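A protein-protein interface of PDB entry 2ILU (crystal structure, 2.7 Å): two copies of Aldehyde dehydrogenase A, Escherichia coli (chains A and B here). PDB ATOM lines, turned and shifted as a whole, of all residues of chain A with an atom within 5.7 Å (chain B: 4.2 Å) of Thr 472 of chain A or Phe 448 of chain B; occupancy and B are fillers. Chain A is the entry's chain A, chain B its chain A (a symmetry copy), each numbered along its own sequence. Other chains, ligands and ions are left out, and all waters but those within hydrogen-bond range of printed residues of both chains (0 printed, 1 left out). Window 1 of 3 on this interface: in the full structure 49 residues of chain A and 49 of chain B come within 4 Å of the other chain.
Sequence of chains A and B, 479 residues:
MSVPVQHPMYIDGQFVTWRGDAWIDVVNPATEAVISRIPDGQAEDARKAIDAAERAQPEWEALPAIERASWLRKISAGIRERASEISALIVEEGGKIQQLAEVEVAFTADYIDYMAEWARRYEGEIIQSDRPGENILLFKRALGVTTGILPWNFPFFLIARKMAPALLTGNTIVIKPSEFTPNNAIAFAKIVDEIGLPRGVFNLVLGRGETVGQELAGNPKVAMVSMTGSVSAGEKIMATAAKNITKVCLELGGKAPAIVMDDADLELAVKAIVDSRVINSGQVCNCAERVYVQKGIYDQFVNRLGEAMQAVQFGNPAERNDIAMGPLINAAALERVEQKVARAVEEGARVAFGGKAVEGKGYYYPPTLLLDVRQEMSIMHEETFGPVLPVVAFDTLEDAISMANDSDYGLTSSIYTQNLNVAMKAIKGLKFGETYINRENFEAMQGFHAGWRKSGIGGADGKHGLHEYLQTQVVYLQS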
ATOM      1  N   LEU A 138      -6.303   6.278  -6.284  1.00  0.00           N
ATOM      2  CA  LEU A 138      -7.109   7.308  -6.890  1.00  0.00           C
ATOM      3  C   LEU A 138      -7.665   6.848  -8.251  1.00  0.00           C
ATOM      4  O   LEU A 138      -6.964   6.932  -9.254  1.00  0.00           O
ATOM      5  CB  LEU A 138      -6.278   8.588  -7.023  1.00  0.00           C
ATOM      6  CG  LEU A 138      -6.988   9.895  -7.379  1.00  0.00           C
ATOM      7  CD1 LEU A 138      -6.261  11.047  -6.703  1.00  0.00           C
ATOM      8  CD2 LEU A 138      -7.025  10.094  -8.884  1.00  0.00           C
ATOM      9  N   PHE A 139      -8.888   6.329  -8.246  1.00  0.00           N
ATOM     10  CA  PHE A 139      -9.511   5.858  -9.474  1.00  0.00           C
ATOM     11  C   PHE A 139     -10.235   6.952 -10.267  1.00  0.00           C
ATOM     12  O   PHE A 139     -10.766   7.878  -9.664  1.00  0.00           O
ATOM     13  CB  PHE A 139     -10.546   4.762  -9.186  1.00  0.00           C
ATOM     14  CG  PHE A 139     -10.010   3.578  -8.435  1.00  0.00           C
ATOM     15  CD1 PHE A 139      -9.745   3.658  -7.074  1.00  0.00           C
ATOM     16  CD2 PHE A 139      -9.814   2.363  -9.083  1.00  0.00           C
ATOM     17  CE1 PHE A 139      -9.296   2.540  -6.371  1.00  0.00           C
ATOM     18  CE2 PHE A 139      -9.364   1.237  -8.387  1.00  0.00           C
ATOM     19  CZ  PHE A 139      -9.105   1.326  -7.029  1.00  0.00           C
ATOM     20  N   LYS A 140     -10.241   6.834 -11.587  1.00  0.00           N
ATOM     21  CA  LYS A 140     -10.961   7.768 -12.438  1.00  0.00           C
ATOM     22  C   LYS A 140     -12.319   7.145 -12.842  1.00  0.00           C
ATOM     23  O   LYS A 140     -12.331   6.181 -13.595  1.00  0.00           O
ATOM     24  CB  LYS A 140     -10.153   8.083 -13.704  1.00  0.00           C
ATOM     25  CG  LYS A 140      -8.843   8.824 -13.485  1.00  0.00           C
ATOM     26  CD  LYS A 140      -9.084  10.228 -12.961  1.00  0.00           C
ATOM     27  CE  LYS A 140      -7.778  10.972 -12.708  1.00  0.00           C
ATOM     28  NZ  LYS A 140      -6.964  11.134 -13.951  1.00  0.00           N
ATOM     29  N   ARG A 141     -13.417   7.644 -12.297  1.00  0.00           N
ATOM     30  CA  ARG A 141     -14.737   7.124 -12.628  1.00  0.00           C
ATOM     31  C   ARG A 141     -15.501   8.069 -13.571  1.00  0.00           C
ATOM     32  O   ARG A 141     -15.081   9.220 -13.741  1.00  0.00           O
ATOM     33  CB  ARG A 141     -15.575   6.948 -11.362  1.00  0.00           C
ATOM     34  CG  ARG A 141     -14.912   6.175 -10.257  1.00  0.00           C
ATOM     35  CD  ARG A 141     -14.888   4.708 -10.562  1.00  0.00           C
ATOM     36  NE  ARG A 141     -14.203   3.959  -9.518  1.00  0.00           N
ATOM     37  CZ  ARG A 141     -13.719   2.737  -9.686  1.00  0.00           C
ATOM     38  NH1 ARG A 141     -13.848   2.131 -10.862  1.00  0.00           N
ATOM     39  NH2 ARG A 141     -13.106   2.124  -8.683  1.00  0.00           N
ATOM     40  N   LEU A 470     -14.234  12.766 -16.601  1.00  0.00           N
ATOM     41  CA  LEU A 470     -13.900  11.848 -15.528  1.00  0.00           C
ATOM     42  C   LEU A 470     -13.857  12.552 -14.173  1.00  0.00           C
ATOM     43  O   LEU A 470     -13.567  13.740 -14.121  1.00  0.00           O
ATOM     44  CB  LEU A 470     -12.534  11.183 -15.766  1.00  0.00           C
ATOM     45  CG  LEU A 470     -12.348  10.066 -16.802  1.00  0.00           C
ATOM     46  CD1 LEU A 470     -10.866   9.807 -16.965  1.00  0.00           C
ATOM     47  CD2 LEU A 470     -13.066   8.791 -16.380  1.00  0.00           C
ATOM     48  N   GLN A 471     -14.196  11.844 -13.114  1.00  0.00           N
ATOM     49  CA  GLN A 471     -14.093  12.413 -11.793  1.00  0.00           C
ATOM     50  C   GLN A 471     -13.277  11.459 -10.916  1.00  0.00           C
ATOM     51  O   GLN A 471     -13.085  10.303 -11.317  1.00  0.00           O
ATOM     52  CB  GLN A 471     -15.471  12.680 -11.197  1.00  0.00           C
ATOM     53  CG  GLN A 471     -16.300  11.464 -10.897  1.00  0.00           C
ATOM     54  CD  GLN A 471     -17.701  11.843 -10.482  1.00  0.00           C
ATOM     55  OE1 GLN A 471     -17.917  12.929  -9.951  1.00  0.00           O
ATOM     56  NE2 GLN A 471     -18.663  10.946 -10.708  1.00  0.00           N
ATOM     57  N   THR A 472     -12.807  11.898  -9.763  1.00  0.00           N
ATOM     58  CA  THR A 472     -11.981  10.999  -9.005  1.00  0.00           C
ATOM     59  C   THR A 472     -12.592  10.347  -7.777  1.00  0.00           C
ATOM     60  O   THR A 472     -13.449  10.928  -7.121  1.00  0.00           O
ATOM     61  CB  THR A 472     -10.693  11.697  -8.591  1.00  0.00           C
ATOM     62  OG1 THR A 472     -10.988  12.660  -7.575  1.00  0.00           O
ATOM     63  CG2 THR A 472     -10.066  12.401  -9.796  1.00  0.00           C
ATOM     64  N   GLN A 473     -12.172   9.119  -7.528  1.00  0.00           N
ATOM     65  CA  GLN A 473     -12.596   8.404  -6.352  1.00  0.00           C
ATOM     66  C   GLN A 473     -11.364   8.009  -5.554  1.00  0.00           C
ATOM     67  O   GLN A 473     -10.674   7.074  -5.956  1.00  0.00           O
ATOM     68  CB  GLN A 473     -13.383   7.147  -6.700  1.00  0.00           C
ATOM     69  CG  GLN A 473     -13.967   6.491  -5.468  1.00  0.00           C
ATOM     70  CD  GLN A 473     -14.473   5.097  -5.731  1.00  0.00           C
ATOM     71  OE1 GLN A 473     -14.419   4.608  -6.860  1.00  0.00           O
ATOM     72  NE2 GLN A 473     -14.972   4.442  -4.687  1.00  0.00           N
ATOM     73  N   VAL A 474     -11.068   8.748  -4.492  1.00  0.00           N
ATOM     74  CA  VAL A 474      -9.908   8.442  -3.675  1.00  0.00           C
ATOM     75  C   VAL A 474     -10.201   7.386  -2.605  1.00  0.00           C
ATOM     76  O   VAL A 474     -11.001   7.640  -1.701  1.00  0.00           O
ATOM     77  CB  VAL A 474      -9.353   9.710  -2.991  1.00  0.00           C
ATOM     78  CG1 VAL A 474      -8.112   9.372  -2.217  1.00  0.00           C
ATOM     79  CG2 VAL A 474      -9.029  10.766  -4.032  1.00  0.00           C
ATOM     80  N   TYR A 476      -8.948   5.133   0.525  1.00  0.00           N
ATOM     81  CA  TYR A 476      -7.958   4.979   1.575  1.00  0.00           C
ATOM     82  C   TYR A 476      -8.014   3.570   2.153  1.00  0.00           C
ATOM     83  O   TYR A 476      -8.725   3.342   3.127  1.00  0.00           O
ATOM     84  CB  TYR A 476      -8.186   5.992   2.701  1.00  0.00           C
ATOM     85  CG  TYR A 476      -7.932   7.432   2.316  1.00  0.00           C
ATOM     86  CD1 TYR A 476      -8.853   8.145   1.540  1.00  0.00           C
ATOM     87  CD2 TYR A 476      -6.772   8.091   2.738  1.00  0.00           C
ATOM     88  CE1 TYR A 476      -8.624   9.480   1.197  1.00  0.00           C
ATOM     89  CE2 TYR A 476      -6.535   9.421   2.400  1.00  0.00           C
ATOM     90  CZ  TYR A 476      -7.462  10.108   1.632  1.00  0.00           C
ATOM     91  OH  TYR A 476      -7.231  11.425   1.299  1.00  0.00           O
ATOM     92  N   GLY B 433     -16.477  10.764  -3.660  1.00  0.00           N
ATOM     93  CA  GLY B 433     -15.155  11.225  -4.029  1.00  0.00           C
ATOM     94  C   GLY B 433     -14.111  10.517  -3.202  1.00  0.00           C
ATOM     95  O   GLY B 433     -12.955  10.395  -3.620  1.00  0.00           O
ATOM     96  N   GLU B 434     -14.534  10.058  -2.026  1.00  0.00           N
ATOM     97  CA  GLU B 434     -13.666   9.350  -1.090  1.00  0.00           C
ATOM     98  C   GLU B 434     -14.317   8.095  -0.452  1.00  0.00           C
ATOM     99  O   GLU B 434     -15.518   8.093  -0.173  1.00  0.00           O
ATOM    100  CB  GLU B 434     -13.222  10.279   0.056  1.00  0.00           C
ATOM    101  CG  GLU B 434     -12.639  11.610  -0.368  1.00  0.00           C
ATOM    102  CD  GLU B 434     -12.321  12.517   0.823  1.00  0.00           C
ATOM    103  OE1 GLU B 434     -13.105  12.512   1.794  1.00  0.00           O
ATOM    104  OE2 GLU B 434     -11.301  13.244   0.781  1.00  0.00           O
ATOM    105  N   GLY B 447      -3.926  13.819  -0.894  1.00  0.00           N
ATOM    106  CA  GLY B 447      -5.010  13.122  -1.562  1.00  0.00           C
ATOM    107  C   GLY B 447      -5.799  14.122  -2.390  1.00  0.00           C
ATOM    108  O   GLY B 447      -5.244  15.103  -2.882  1.00  0.00           O
ATOM    109  N   PHE B 448      -7.093  13.895  -2.561  1.00  0.00           N
ATOM    110  CA  PHE B 448      -7.907  14.830  -3.324  1.00  0.00           C
ATOM    111  C   PHE B 448      -9.353  14.926  -2.805  1.00  0.00           C
ATOM    112  O   PHE B 448     -10.163  14.032  -3.060  1.00  0.00           O
ATOM    113  CB  PHE B 448      -7.894  14.462  -4.815  1.00  0.00           C
ATOM    114  CG  PHE B 448      -8.550  15.491  -5.711  1.00  0.00           C
ATOM    115  CD1 PHE B 448      -8.315  16.856  -5.529  1.00  0.00           C
ATOM    116  CD2 PHE B 448      -9.381  15.094  -6.756  1.00  0.00           C
ATOM    117  CE1 PHE B 448      -8.894  17.814  -6.375  1.00  0.00           C
ATOM    118  CE2 PHE B 448      -9.970  16.041  -7.613  1.00  0.00           C
ATOM    119  CZ  PHE B 448      -9.722  17.407  -7.418  1.00  0.00           C
ATOM    120  N   HIS B 449      -9.633  15.989  -2.064  1.00  0.00           N
ATOM    121  CA  HIS B 449     -10.953  16.220  -1.503  1.00  0.00           C
ATOM    122  C   HIS B 449     -11.935  16.842  -2.532  1.00  0.00           C
ATOM    123  O   HIS B 449     -11.938  18.065  -2.713  1.00  0.00           O
ATOM    124  CB  HIS B 449     -10.809  17.133  -0.284  1.00  0.00           C
ATOM    125  CG  HIS B 449     -11.935  17.027   0.698  1.00  0.00           C
ATOM    126  ND1 HIS B 449     -12.258  15.847   1.333  1.00  0.00           N
ATOM    127  CD2 HIS B 449     -12.783  17.962   1.186  1.00  0.00           C
ATOM    128  CE1 HIS B 449     -13.254  16.062   2.176  1.00  0.00           C
ATOM    129  NE2 HIS B 449     -13.590  17.336   2.105  1.00  0.00           N
ATOM    130  N   ALA B 450     -12.721  16.000  -3.190  1.00  0.00           N
ATOM    131  CA  ALA B 450     -13.678  16.457  -4.196  1.00  0.00           C
ATOM    132  C   ALA B 450     -14.968  15.645  -4.178  1.00  0.00           C
ATOM    133  O   ALA B 450     -14.897  14.423  -4.261  1.00  0.00           O
ATOM    134  CB  ALA B 450     -13.051  16.393  -5.582  1.00  0.00           C
ATOM    135  N   TRP B 452     -18.826  14.284  -5.402  1.00  0.00           N
ATOM    136  CA  TRP B 452     -19.699  14.018  -6.528  1.00  0.00           C
ATOM    137  C   TRP B 452     -21.083  14.688  -6.335  1.00  0.00           C
ATOM    138  O   TRP B 452     -21.388  15.115  -5.217  1.00  0.00           O
ATOM    139  CB  TRP B 452     -19.897  12.509  -6.692  1.00  0.00           C
ATOM    140  CG  TRP B 452     -18.669  11.748  -7.095  1.00  0.00           C
ATOM    141  CD1 TRP B 452     -17.375  12.121  -6.913  1.00  0.00           C
ATOM    142  CD2 TRP B 452     -18.631  10.448  -7.689  1.00  0.00           C
ATOM    143  NE1 TRP B 452     -16.525  11.136  -7.353  1.00  0.00           N
ATOM    144  CE2 TRP B 452     -17.270  10.094  -7.834  1.00  0.00           C
ATOM    145  CE3 TRP B 452     -19.615   9.542  -8.113  1.00  0.00           C
ATOM    146  CZ2 TRP B 452     -16.863   8.874  -8.383  1.00  0.00           C
ATOM    147  CZ3 TRP B 452     -19.213   8.326  -8.661  1.00  0.00           C
ATOM    148  CH2 TRP B 452     -17.842   8.005  -8.791  1.00  0.00           C
ATOM    149  N   GLY B 459     -11.940  20.698  -6.619  1.00  0.00           N
ATOM    150  CA  GLY B 459     -11.588  20.046  -5.377  1.00  0.00           C
ATOM    151  C   GLY B 459     -10.413  20.704  -4.695  1.00  0.00           C
ATOM    152  O   GLY B 459     -10.019  21.824  -5.041  1.00  0.00           O
ATOM    153  N   ALA B 460      -9.849  19.997  -3.722  1.00  0.00           N
ATOM    154  CA  ALA B 460      -8.718  20.507  -2.976  1.00  0.00           C
ATOM    155  C   ALA B 460      -7.685  19.452  -2.572  1.00  0.00           C
ATOM    156  O   ALA B 460      -7.961  18.257  -2.645  1.00  0.00           O
ATOM    157  CB  ALA B 460      -9.211  21.235  -1.729  1.00  0.00           C
ATOM    158  N   ASP B 461      -6.528  19.926  -2.136  1.00  0.00           N
ATOM    159  CA  ASP B 461      -5.433  19.079  -1.693  1.00  0.00           C
ATOM    160  C   ASP B 461      -4.706  18.303  -2.815  1.00  0.00           C
ATOM    161  O   ASP B 461      -5.265  18.084  -3.899  1.00  0.00           O
ATOM    162  CB  ASP B 461      -5.917  18.083  -0.622  1.00  0.00           C
ATOM    163  CG  ASP B 461      -6.843  18.719   0.408  1.00  0.00           C
ATOM    164  OD1 ASP B 461      -6.680  19.917   0.712  1.00  0.00           O
ATOM    165  OD2 ASP B 461      -7.734  18.017   0.929  1.00  0.00           O
ATOM    166  N   HIS B 464      -3.974  17.476  -7.739  1.00  0.00           N
ATOM    167  CA  HIS B 464      -5.173  17.960  -8.399  1.00  0.00           C
ATOM    168  C   HIS B 464      -5.737  19.196  -7.721  1.00  0.00           C
ATOM    169  O   HIS B 464      -6.290  20.054  -8.397  1.00  0.00           O
ATOM    170  CB  HIS B 464      -6.226  16.852  -8.471  1.00  0.00           C
ATOM    171  CG  HIS B 464      -5.735  15.628  -9.173  1.00  0.00           C
ATOM    172  ND1 HIS B 464      -5.188  15.675 -10.439  1.00  0.00           N
ATOM    173  CD2 HIS B 464      -5.632  14.342  -8.765  1.00  0.00           C
ATOM    174  CE1 HIS B 464      -4.765  14.469 -10.775  1.00  0.00           C
ATOM    175  NE2 HIS B 464      -5.022  13.644  -9.776  1.00  0.00           N
ATOM    176  N   GLY B 465      -5.593  19.278  -6.407  1.00  0.00           N
ATOM    177  CA  GLY B 465      -6.055  20.463  -5.715  1.00  0.00           C
ATOM    178  C   GLY B 465      -5.199  21.620  -6.200  1.00  0.00           C
ATOM    179  O   GLY B 465      -5.705  22.688  -6.510  1.00  0.00           O
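Of the 10 printed residues of chain A, 7 touch a printed residue of chain B.
Hydrophobic or aromatic side chains of chain A that line the printed part of chain B: Leu 138, Val 474 and Tyr 476.
Among the printed residues, no Asp or Glu carboxylate lies within 4 Å of a Lys or Arg side-chain nitrogen of the other chain.
N of Val 474 of chain A lies within hydrogen-bond range of O of Gly 433 of chain B (2.7 Å).
The indole nitrogen of Trp 452 of chain B lies within hydrogen-bond range of the backbone carbonyl oxygen of Thr 472 of chain A, at 3.1 Å.
The side-chain amide oxygen of Gln 471 of chain A sits close to the indole nitrogen of Trp 452 of chain B, 3.4 Å away.
Leu 138 of chain A touches His 464 of chain B.
Arg 141 of chain A touches Trp 452 of chain B.
CA of Gly 433 of chain B touches O of Thr 472 of chain A, at 3.5 Å.
Thr 472 of chain A touches Phe 448 of chain B (OG1 to CD2, 3.0 Å).
Gln 473 of chain A touches Gly 433 of chain B (CA to O, 3.4 Å).
Val 474 of chain A touches Glu 434 of chain B (O to CA, 3.2 Å).
Phe 448 of chain B touches Val 474 of chain A.
Tyr 476 of chain A touches Gly 447 of chain B.
Of the printed residues of chain B, Arg 141 of chain A touches Trp 452.
Of the printed residues of chain B, Gln 471 of chain A touches Trp 452.
Of chain B, only Gly 433, Phe 448 and Trp 452 come within 4 Å of Thr 472 of chain A.
Of the printed residues of chain A, Glu 434 of chain B touches Val 474 (3.2 Å).
Of the printed residues of chain A, His 464 of chain B touches Leu 138.
The nearest printed residue of chain B that does not touch Thr 472 of chain A is Ala 450 of chain B (4.7 Å).
The side-chain carboxylate (OE2) of Glu 434 of chain B is in hydrogen-bond range of a ring nitrogen (ND1) of His 449 of chain B.
The backbone NH of Gln 471 of chain A sits at hydrogen-bond distance from the backbone carbonyl oxygen of Arg 141 of chain A, 2.8 Å away.
O of Phe 139 of chain A sits at hydrogen-bond distance from N of Gln 473 of chain A, at 2.8 Å.
NE of Arg 141 of chain A lies within hydrogen-bond range of OE1 of Gln 473 of chain A, 2.7 Å away.
No position is printed for both chains.
Of the 11 pairs that touch across the chains among the printed residues, none has its exchanged pair printed and touching as well.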
